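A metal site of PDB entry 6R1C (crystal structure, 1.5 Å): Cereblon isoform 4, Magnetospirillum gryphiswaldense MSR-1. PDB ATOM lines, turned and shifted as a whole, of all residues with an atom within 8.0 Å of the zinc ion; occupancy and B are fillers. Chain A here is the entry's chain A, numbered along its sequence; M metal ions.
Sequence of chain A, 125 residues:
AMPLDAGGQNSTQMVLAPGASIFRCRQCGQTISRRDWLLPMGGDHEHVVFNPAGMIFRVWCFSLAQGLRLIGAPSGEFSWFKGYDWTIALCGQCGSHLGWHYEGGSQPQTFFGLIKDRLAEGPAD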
ATOM      1  N   ARG A  24     -17.050 -18.699 -11.430  1.00  0.00           N
ATOM      2  CA  ARG A  24     -16.249 -17.860 -10.572  1.00  0.00           C
ATOM      3  C   ARG A  24     -15.078 -18.641  -9.982  1.00  0.00           C
ATOM      4  O   ARG A  24     -15.136 -19.845  -9.896  1.00  0.00           O
ATOM      5  CB  ARG A  24     -17.128 -17.324  -9.434  1.00  0.00           C
ATOM      6  CG  ARG A  24     -18.193 -16.363  -9.926  1.00  0.00           C
ATOM      7  CD  ARG A  24     -19.002 -15.754  -8.763  1.00  0.00           C
ATOM      8  NE  ARG A  24     -19.918 -14.788  -9.309  1.00  0.00           N
ATOM      9  CZ  ARG A  24     -19.600 -13.581  -9.749  1.00  0.00           C
ATOM     10  NH1 ARG A  24     -18.379 -13.076  -9.607  1.00  0.00           N
ATOM     11  NH2 ARG A  24     -20.534 -12.843 -10.319  1.00  0.00           N
ATOM     12  N   CYS A  25     -14.028 -17.944  -9.551  1.00  0.00           N
ATOM     13  CA  CYS A  25     -12.956 -18.601  -8.822  1.00  0.00           C
ATOM     14  C   CYS A  25     -13.533 -19.216  -7.534  1.00  0.00           C
ATOM     15  O   CYS A  25     -14.220 -18.515  -6.778  1.00  0.00           O
ATOM     16  CB  CYS A  25     -11.882 -17.605  -8.472  1.00  0.00           C
ATOM     17  SG  CYS A  25     -10.580 -18.306  -7.428  1.00  0.00           S
ATOM     18  N   ARG A  26     -13.276 -20.500  -7.317  1.00  0.00           N
ATOM     19  CA  ARG A  26     -13.757 -21.193  -6.133  1.00  0.00           C
ATOM     20  C   ARG A  26     -13.255 -20.614  -4.805  1.00  0.00           C
ATOM     21  O   ARG A  26     -13.941 -20.694  -3.777  1.00  0.00           O
ATOM     22  CB  ARG A  26     -13.380 -22.663  -6.234  1.00  0.00           C
ATOM     23  CG  ARG A  26     -13.822 -23.501  -5.078  1.00  0.00           C
ATOM     24  CD  ARG A  26     -13.437 -24.927  -5.330  1.00  0.00           C
ATOM     25  NE  ARG A  26     -13.647 -25.705  -4.131  1.00  0.00           N
ATOM     26  CZ  ARG A  26     -13.445 -27.005  -4.020  1.00  0.00           C
ATOM     27  NH1 ARG A  26     -13.062 -27.733  -5.063  1.00  0.00           N
ATOM     28  NH2 ARG A  26     -13.652 -27.585  -2.849  1.00  0.00           N
ATOM     29  N   GLN A  27     -12.041 -20.070  -4.838  1.00  0.00           N
ATOM     30  CA  GLN A  27     -11.402 -19.539  -3.622  1.00  0.00           C
ATOM     31  C   GLN A  27     -11.868 -18.151  -3.224  1.00  0.00           C
ATOM     32  O   GLN A  27     -11.934 -17.856  -2.043  1.00  0.00           O
ATOM     33  CB  GLN A  27      -9.872 -19.607  -3.758  1.00  0.00           C
ATOM     34  CG  GLN A  27      -9.352 -20.986  -4.005  1.00  0.00           C
ATOM     35  CD  GLN A  27      -9.832 -21.972  -2.988  1.00  0.00           C
ATOM     36  OE1 GLN A  27      -9.893 -21.701  -1.788  1.00  0.00           O
ATOM     37  NE2 GLN A  27     -10.182 -23.155  -3.455  1.00  0.00           N
ATOM     38  N   CYS A  28     -12.176 -17.280  -4.172  1.00  0.00           N
ATOM     39  CA  CYS A  28     -12.485 -15.876  -3.861  1.00  0.00           C
ATOM     40  C   CYS A  28     -13.707 -15.294  -4.545  1.00  0.00           C
ATOM     41  O   CYS A  28     -14.114 -14.193  -4.217  1.00  0.00           O
ATOM     42  CB  CYS A  28     -11.262 -15.014  -4.174  1.00  0.00           C
ATOM     43  SG  CYS A  28     -11.032 -14.766  -5.946  1.00  0.00           S
ATOM     44  N   GLY A  29     -14.275 -15.953  -5.558  1.00  0.00           N
ATOM     45  CA  GLY A  29     -15.429 -15.436  -6.237  1.00  0.00           C
ATOM     46  C   GLY A  29     -15.246 -14.544  -7.436  1.00  0.00           C
ATOM     47  O   GLY A  29     -16.237 -14.086  -8.053  1.00  0.00           O
ATOM     48  N   GLN A  30     -13.990 -14.257  -7.807  1.00  0.00           N
ATOM     49  CA  GLN A  30     -13.718 -13.482  -9.020  1.00  0.00           C
ATOM     50  C   GLN A  30     -14.461 -14.073 -10.225  1.00  0.00           C
ATOM     51  O   GLN A  30     -14.426 -15.257 -10.418  1.00  0.00           O
ATOM     52  CB  GLN A  30     -12.195 -13.511  -9.332  1.00  0.00           C
ATOM     53  CG  GLN A  30     -11.773 -12.861 -10.639  1.00  0.00           C
ATOM     54  CD  GLN A  30     -12.228 -11.416 -10.782  1.00  0.00           C
ATOM     55  OE1 GLN A  30     -12.121 -10.658  -9.854  1.00  0.00           O
ATOM     56  NE2 GLN A  30     -12.715 -11.020 -11.956  1.00  0.00           N
ATOM     57  N   THR A  31     -15.094 -13.228 -11.003  1.00  0.00           N
ATOM     58  CA  THR A  31     -15.773 -13.701 -12.215  1.00  0.00           C
ATOM     59  C   THR A  31     -14.726 -14.140 -13.233  1.00  0.00           C
ATOM     60  O   THR A  31     -13.789 -13.393 -13.492  1.00  0.00           O
ATOM     61  CB  THR A  31     -16.692 -12.633 -12.815  1.00  0.00           C
ATOM     62  OG1 THR A  31     -17.549 -13.225 -13.785  1.00  0.00           O
ATOM     63  CG2 THR A  31     -15.971 -11.450 -13.388  1.00  0.00           C
ATOM     64  N   ILE A  32     -14.870 -15.344 -13.767  1.00  0.00           N
ATOM     65  CA  ILE A  32     -13.861 -15.926 -14.679  1.00  0.00           C
ATOM     66  C   ILE A  32     -14.419 -16.266 -16.075  1.00  0.00           C
ATOM     67  O   ILE A  32     -13.809 -15.905 -17.081  1.00  0.00           O
ATOM     68  CB  ILE A  32     -13.218 -17.214 -14.102  1.00  0.00           C
ATOM     69  CG1 ILE A  32     -12.582 -16.970 -12.753  1.00  0.00           C
ATOM     70  CG2 ILE A  32     -12.173 -17.782 -15.083  1.00  0.00           C
ATOM     71  CD1 ILE A  32     -11.426 -15.987 -12.725  1.00  0.00           C
ATOM     72  N   GLY A  67     -10.749 -11.953 -15.725  1.00  0.00           N
ATOM     73  CA  GLY A  67     -10.432 -12.043 -14.295  1.00  0.00           C
ATOM     74  C   GLY A  67      -9.188 -12.821 -13.950  1.00  0.00           C
ATOM     75  O   GLY A  67      -8.912 -13.056 -12.786  1.00  0.00           O
ATOM     76  N   LEU A  68      -8.424 -13.246 -14.952  1.00  0.00           N
ATOM     77  CA  LEU A  68      -7.224 -14.021 -14.766  1.00  0.00           C
ATOM     78  C   LEU A  68      -6.033 -13.108 -14.891  1.00  0.00           C
ATOM     79  O   LEU A  68      -6.164 -11.943 -15.265  1.00  0.00           O
ATOM     80  CB  LEU A  68      -7.107 -15.115 -15.824  1.00  0.00           C
ATOM     81  CG  LEU A  68      -8.248 -16.130 -15.829  1.00  0.00           C
ATOM     82  CD1 LEU A  68      -8.332 -16.834 -17.175  1.00  0.00           C
ATOM     83  CD2 LEU A  68      -8.128 -17.098 -14.646  1.00  0.00           C
ATOM     84  N   LEU A  90      -3.583 -17.546 -13.583  1.00  0.00           N
ATOM     85  CA  LEU A  90      -3.953 -17.467 -12.168  1.00  0.00           C
ATOM     86  C   LEU A  90      -5.209 -16.640 -12.064  1.00  0.00           C
ATOM     87  O   LEU A  90      -5.452 -15.773 -12.899  1.00  0.00           O
ATOM     88  CB  LEU A  90      -2.834 -16.781 -11.386  1.00  0.00           C
ATOM     89  CG  LEU A  90      -1.447 -17.413 -11.479  1.00  0.00           C
ATOM     90  CD1 LEU A  90      -0.511 -16.639 -10.565  1.00  0.00           C
ATOM     91  CD2 LEU A  90      -1.488 -18.887 -11.090  1.00  0.00           C
ATOM     92  N   CYS A  91      -5.976 -16.882 -11.017  1.00  0.00           N
ATOM     93  CA  CYS A  91      -7.008 -15.918 -10.634  1.00  0.00           C
ATOM     94  C   CYS A  91      -6.333 -14.565 -10.405  1.00  0.00           C
ATOM     95  O   CYS A  91      -5.344 -14.451  -9.654  1.00  0.00           O
ATOM     96  CB  CYS A  91      -7.703 -16.343  -9.372  1.00  0.00           C
ATOM     97  SG  CYS A  91      -8.965 -15.148  -8.841  1.00  0.00           S
ATOM     98  N   GLY A  92      -6.830 -13.535 -11.079  1.00  0.00           N
ATOM     99  CA  GLY A  92      -6.273 -12.200 -10.983  1.00  0.00           C
ATOM    100  C   GLY A  92      -6.486 -11.561  -9.645  1.00  0.00           C
ATOM    101  O   GLY A  92      -5.807 -10.604  -9.323  1.00  0.00           O
ATOM    102  N   GLN A  93      -7.446 -12.065  -8.887  1.00  0.00           N
ATOM    103  CA  GLN A  93      -7.794 -11.515  -7.598  1.00  0.00           C
ATOM    104  C   GLN A  93      -6.972 -12.190  -6.492  1.00  0.00           C
ATOM    105  O   GLN A  93      -6.251 -11.542  -5.763  1.00  0.00           O
ATOM    106  CB  GLN A  93      -9.288 -11.657  -7.379  1.00  0.00           C
ATOM    107  CG  GLN A  93      -9.783 -11.065  -6.056  1.00  0.00           C
ATOM    108  CD  GLN A  93     -11.257 -10.715  -6.101  1.00  0.00           C
ATOM    109  OE1 GLN A  93     -11.616  -9.603  -6.412  1.00  0.00           O
ATOM    110  NE2 GLN A  93     -12.110 -11.695  -5.872  1.00  0.00           N
ATOM    111  N   CYS A  94      -7.051 -13.524  -6.399  1.00  0.00           N
ATOM    112  CA  CYS A  94      -6.432 -14.245  -5.273  1.00  0.00           C
ATOM    113  C   CYS A  94      -5.166 -15.061  -5.590  1.00  0.00           C
ATOM    114  O   CYS A  94      -4.534 -15.548  -4.677  1.00  0.00           O
ATOM    115  CB  CYS A  94      -7.450 -15.127  -4.618  1.00  0.00           C
ATOM    116  SG  CYS A  94      -7.776 -16.725  -5.461  1.00  0.00           S
ATOM    117  N   GLY A  95      -4.850 -15.222  -6.875  1.00  0.00           N
ATOM    118  CA  GLY A  95      -3.660 -15.951  -7.282  1.00  0.00           C
ATOM    119  C   GLY A  95      -3.801 -17.444  -7.405  1.00  0.00           C
ATOM    120  O   GLY A  95      -2.831 -18.117  -7.726  1.00  0.00           O
ATOM    121  N   SER A  96      -4.996 -17.994  -7.153  1.00  0.00           N
ATOM    122  CA  SER A  96      -5.265 -19.432  -7.317  1.00  0.00           C
ATOM    123  C   SER A  96      -4.931 -19.853  -8.753  1.00  0.00           C
ATOM    124  O   SER A  96      -5.273 -19.149  -9.703  1.00  0.00           O
ATOM    125  CB  SER A  96      -6.732 -19.730  -7.039  1.00  0.00           C
ATOM    126  OG  SER A  96      -7.073 -21.097  -7.240  1.00  0.00           O
ATOM    127  N   HIS A  97      -4.269 -20.994  -8.912  1.00  0.00           N
ATOM    128  CA  HIS A  97      -3.995 -21.459 -10.267  1.00  0.00           C
ATOM    129  C   HIS A  97      -5.257 -22.054 -10.866  1.00  0.00           C
ATOM    130  O   HIS A  97      -5.698 -23.087 -10.436  1.00  0.00           O
ATOM    131  CB  HIS A  97      -2.874 -22.485 -10.240  1.00  0.00           C
ATOM    132  CG  HIS A  97      -2.593 -23.050 -11.577  1.00  0.00           C
ATOM    133  ND1 HIS A  97      -2.073 -24.308 -11.739  1.00  0.00           N
ATOM    134  CD2 HIS A  97      -2.722 -22.512 -12.816  1.00  0.00           C
ATOM    135  CE1 HIS A  97      -1.918 -24.527 -13.028  1.00  0.00           C
ATOM    136  NE2 HIS A  97      -2.327 -23.470 -13.705  1.00  0.00           N
ATOM    137  N   LEU A  98      -5.855 -21.390 -11.848  1.00  0.00           N
ATOM    138  CA  LEU A  98      -7.115 -21.814 -12.443  1.00  0.00           C
ATOM    139  C   LEU A  98      -6.993 -22.576 -13.755  1.00  0.00           C
ATOM    140  O   LEU A  98      -7.943 -23.231 -14.157  1.00  0.00           O
ATOM    141  CB  LEU A  98      -8.056 -20.624 -12.628  1.00  0.00           C
ATOM    142  CG  LEU A  98      -8.485 -19.940 -11.316  1.00  0.00           C
ATOM    143  CD1 LEU A  98      -9.540 -18.880 -11.614  1.00  0.00           C
ATOM    144  CD2 LEU A  98      -9.012 -20.880 -10.237  1.00  0.00           C
ATOM    145  N   ARG A 118     -11.682 -26.140  -9.740  1.00  0.00           N
ATOM    146  CA  ARG A 118     -11.200 -24.886  -9.161  1.00  0.00           C
ATOM    147  C   ARG A 118     -12.116 -23.717  -9.434  1.00  0.00           C
ATOM    148  O   ARG A 118     -11.819 -22.551  -9.050  1.00  0.00           O
ATOM    149  CB  ARG A 118      -9.774 -24.614  -9.620  1.00  0.00           C
ATOM    150  CG  ARG A 118      -8.847 -25.768  -9.211  1.00  0.00           C
ATOM    151  CD  ARG A 118      -7.394 -25.504  -9.354  1.00  0.00           C
ATOM    152  NE  ARG A 118      -6.580 -26.673  -9.092  1.00  0.00           N
ATOM    153  CZ  ARG A 118      -5.252 -26.694  -9.169  1.00  0.00           C
ATOM    154  NH1 ARG A 118      -4.555 -25.606  -9.493  1.00  0.00           N
ATOM    155  NH2 ARG A 118      -4.591 -27.834  -8.918  1.00  0.00           N
HETATM  156 ZN    ZN M   1      -9.590 -16.308  -6.841  1.00  0.00          ZN
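The backbone carbonyl oxygen (O) of Gln 30 sits at hydrogen-bond distance from the backbone NH (N) of Cys 25 (2.9 Å).
SG of Cys 94 sits close to N of Ser 96, 3.5 Å away.
NE2 of Gln 93 sits close to SG of Cys 28 (3.3 Å).
SG of Cys 25 sits close to N of Gln 27, at 3.5 Å.
N of Gln 30 lies close to SG of Cys 28 (3.5 Å).
O of Ser 96 lies within hydrogen-bond range of N of Cys 91.
SG of Cys 91 lies close to N of Gln 93 (3.4 Å).
The nearest printed residue that does not touch the zinc ion is Ser 96 (4.5 Å).
The zinc ion is bound by the side-chain sulfur (SG) of Cys 28 (2.3 Å), the side-chain sulfur (SG) of Cys 25 (2.3 Å), the side-chain sulfur (SG) of Cys 94 (2.3 Å) and the side-chain sulfur (SG) of Cys 91 (2.4 Å).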
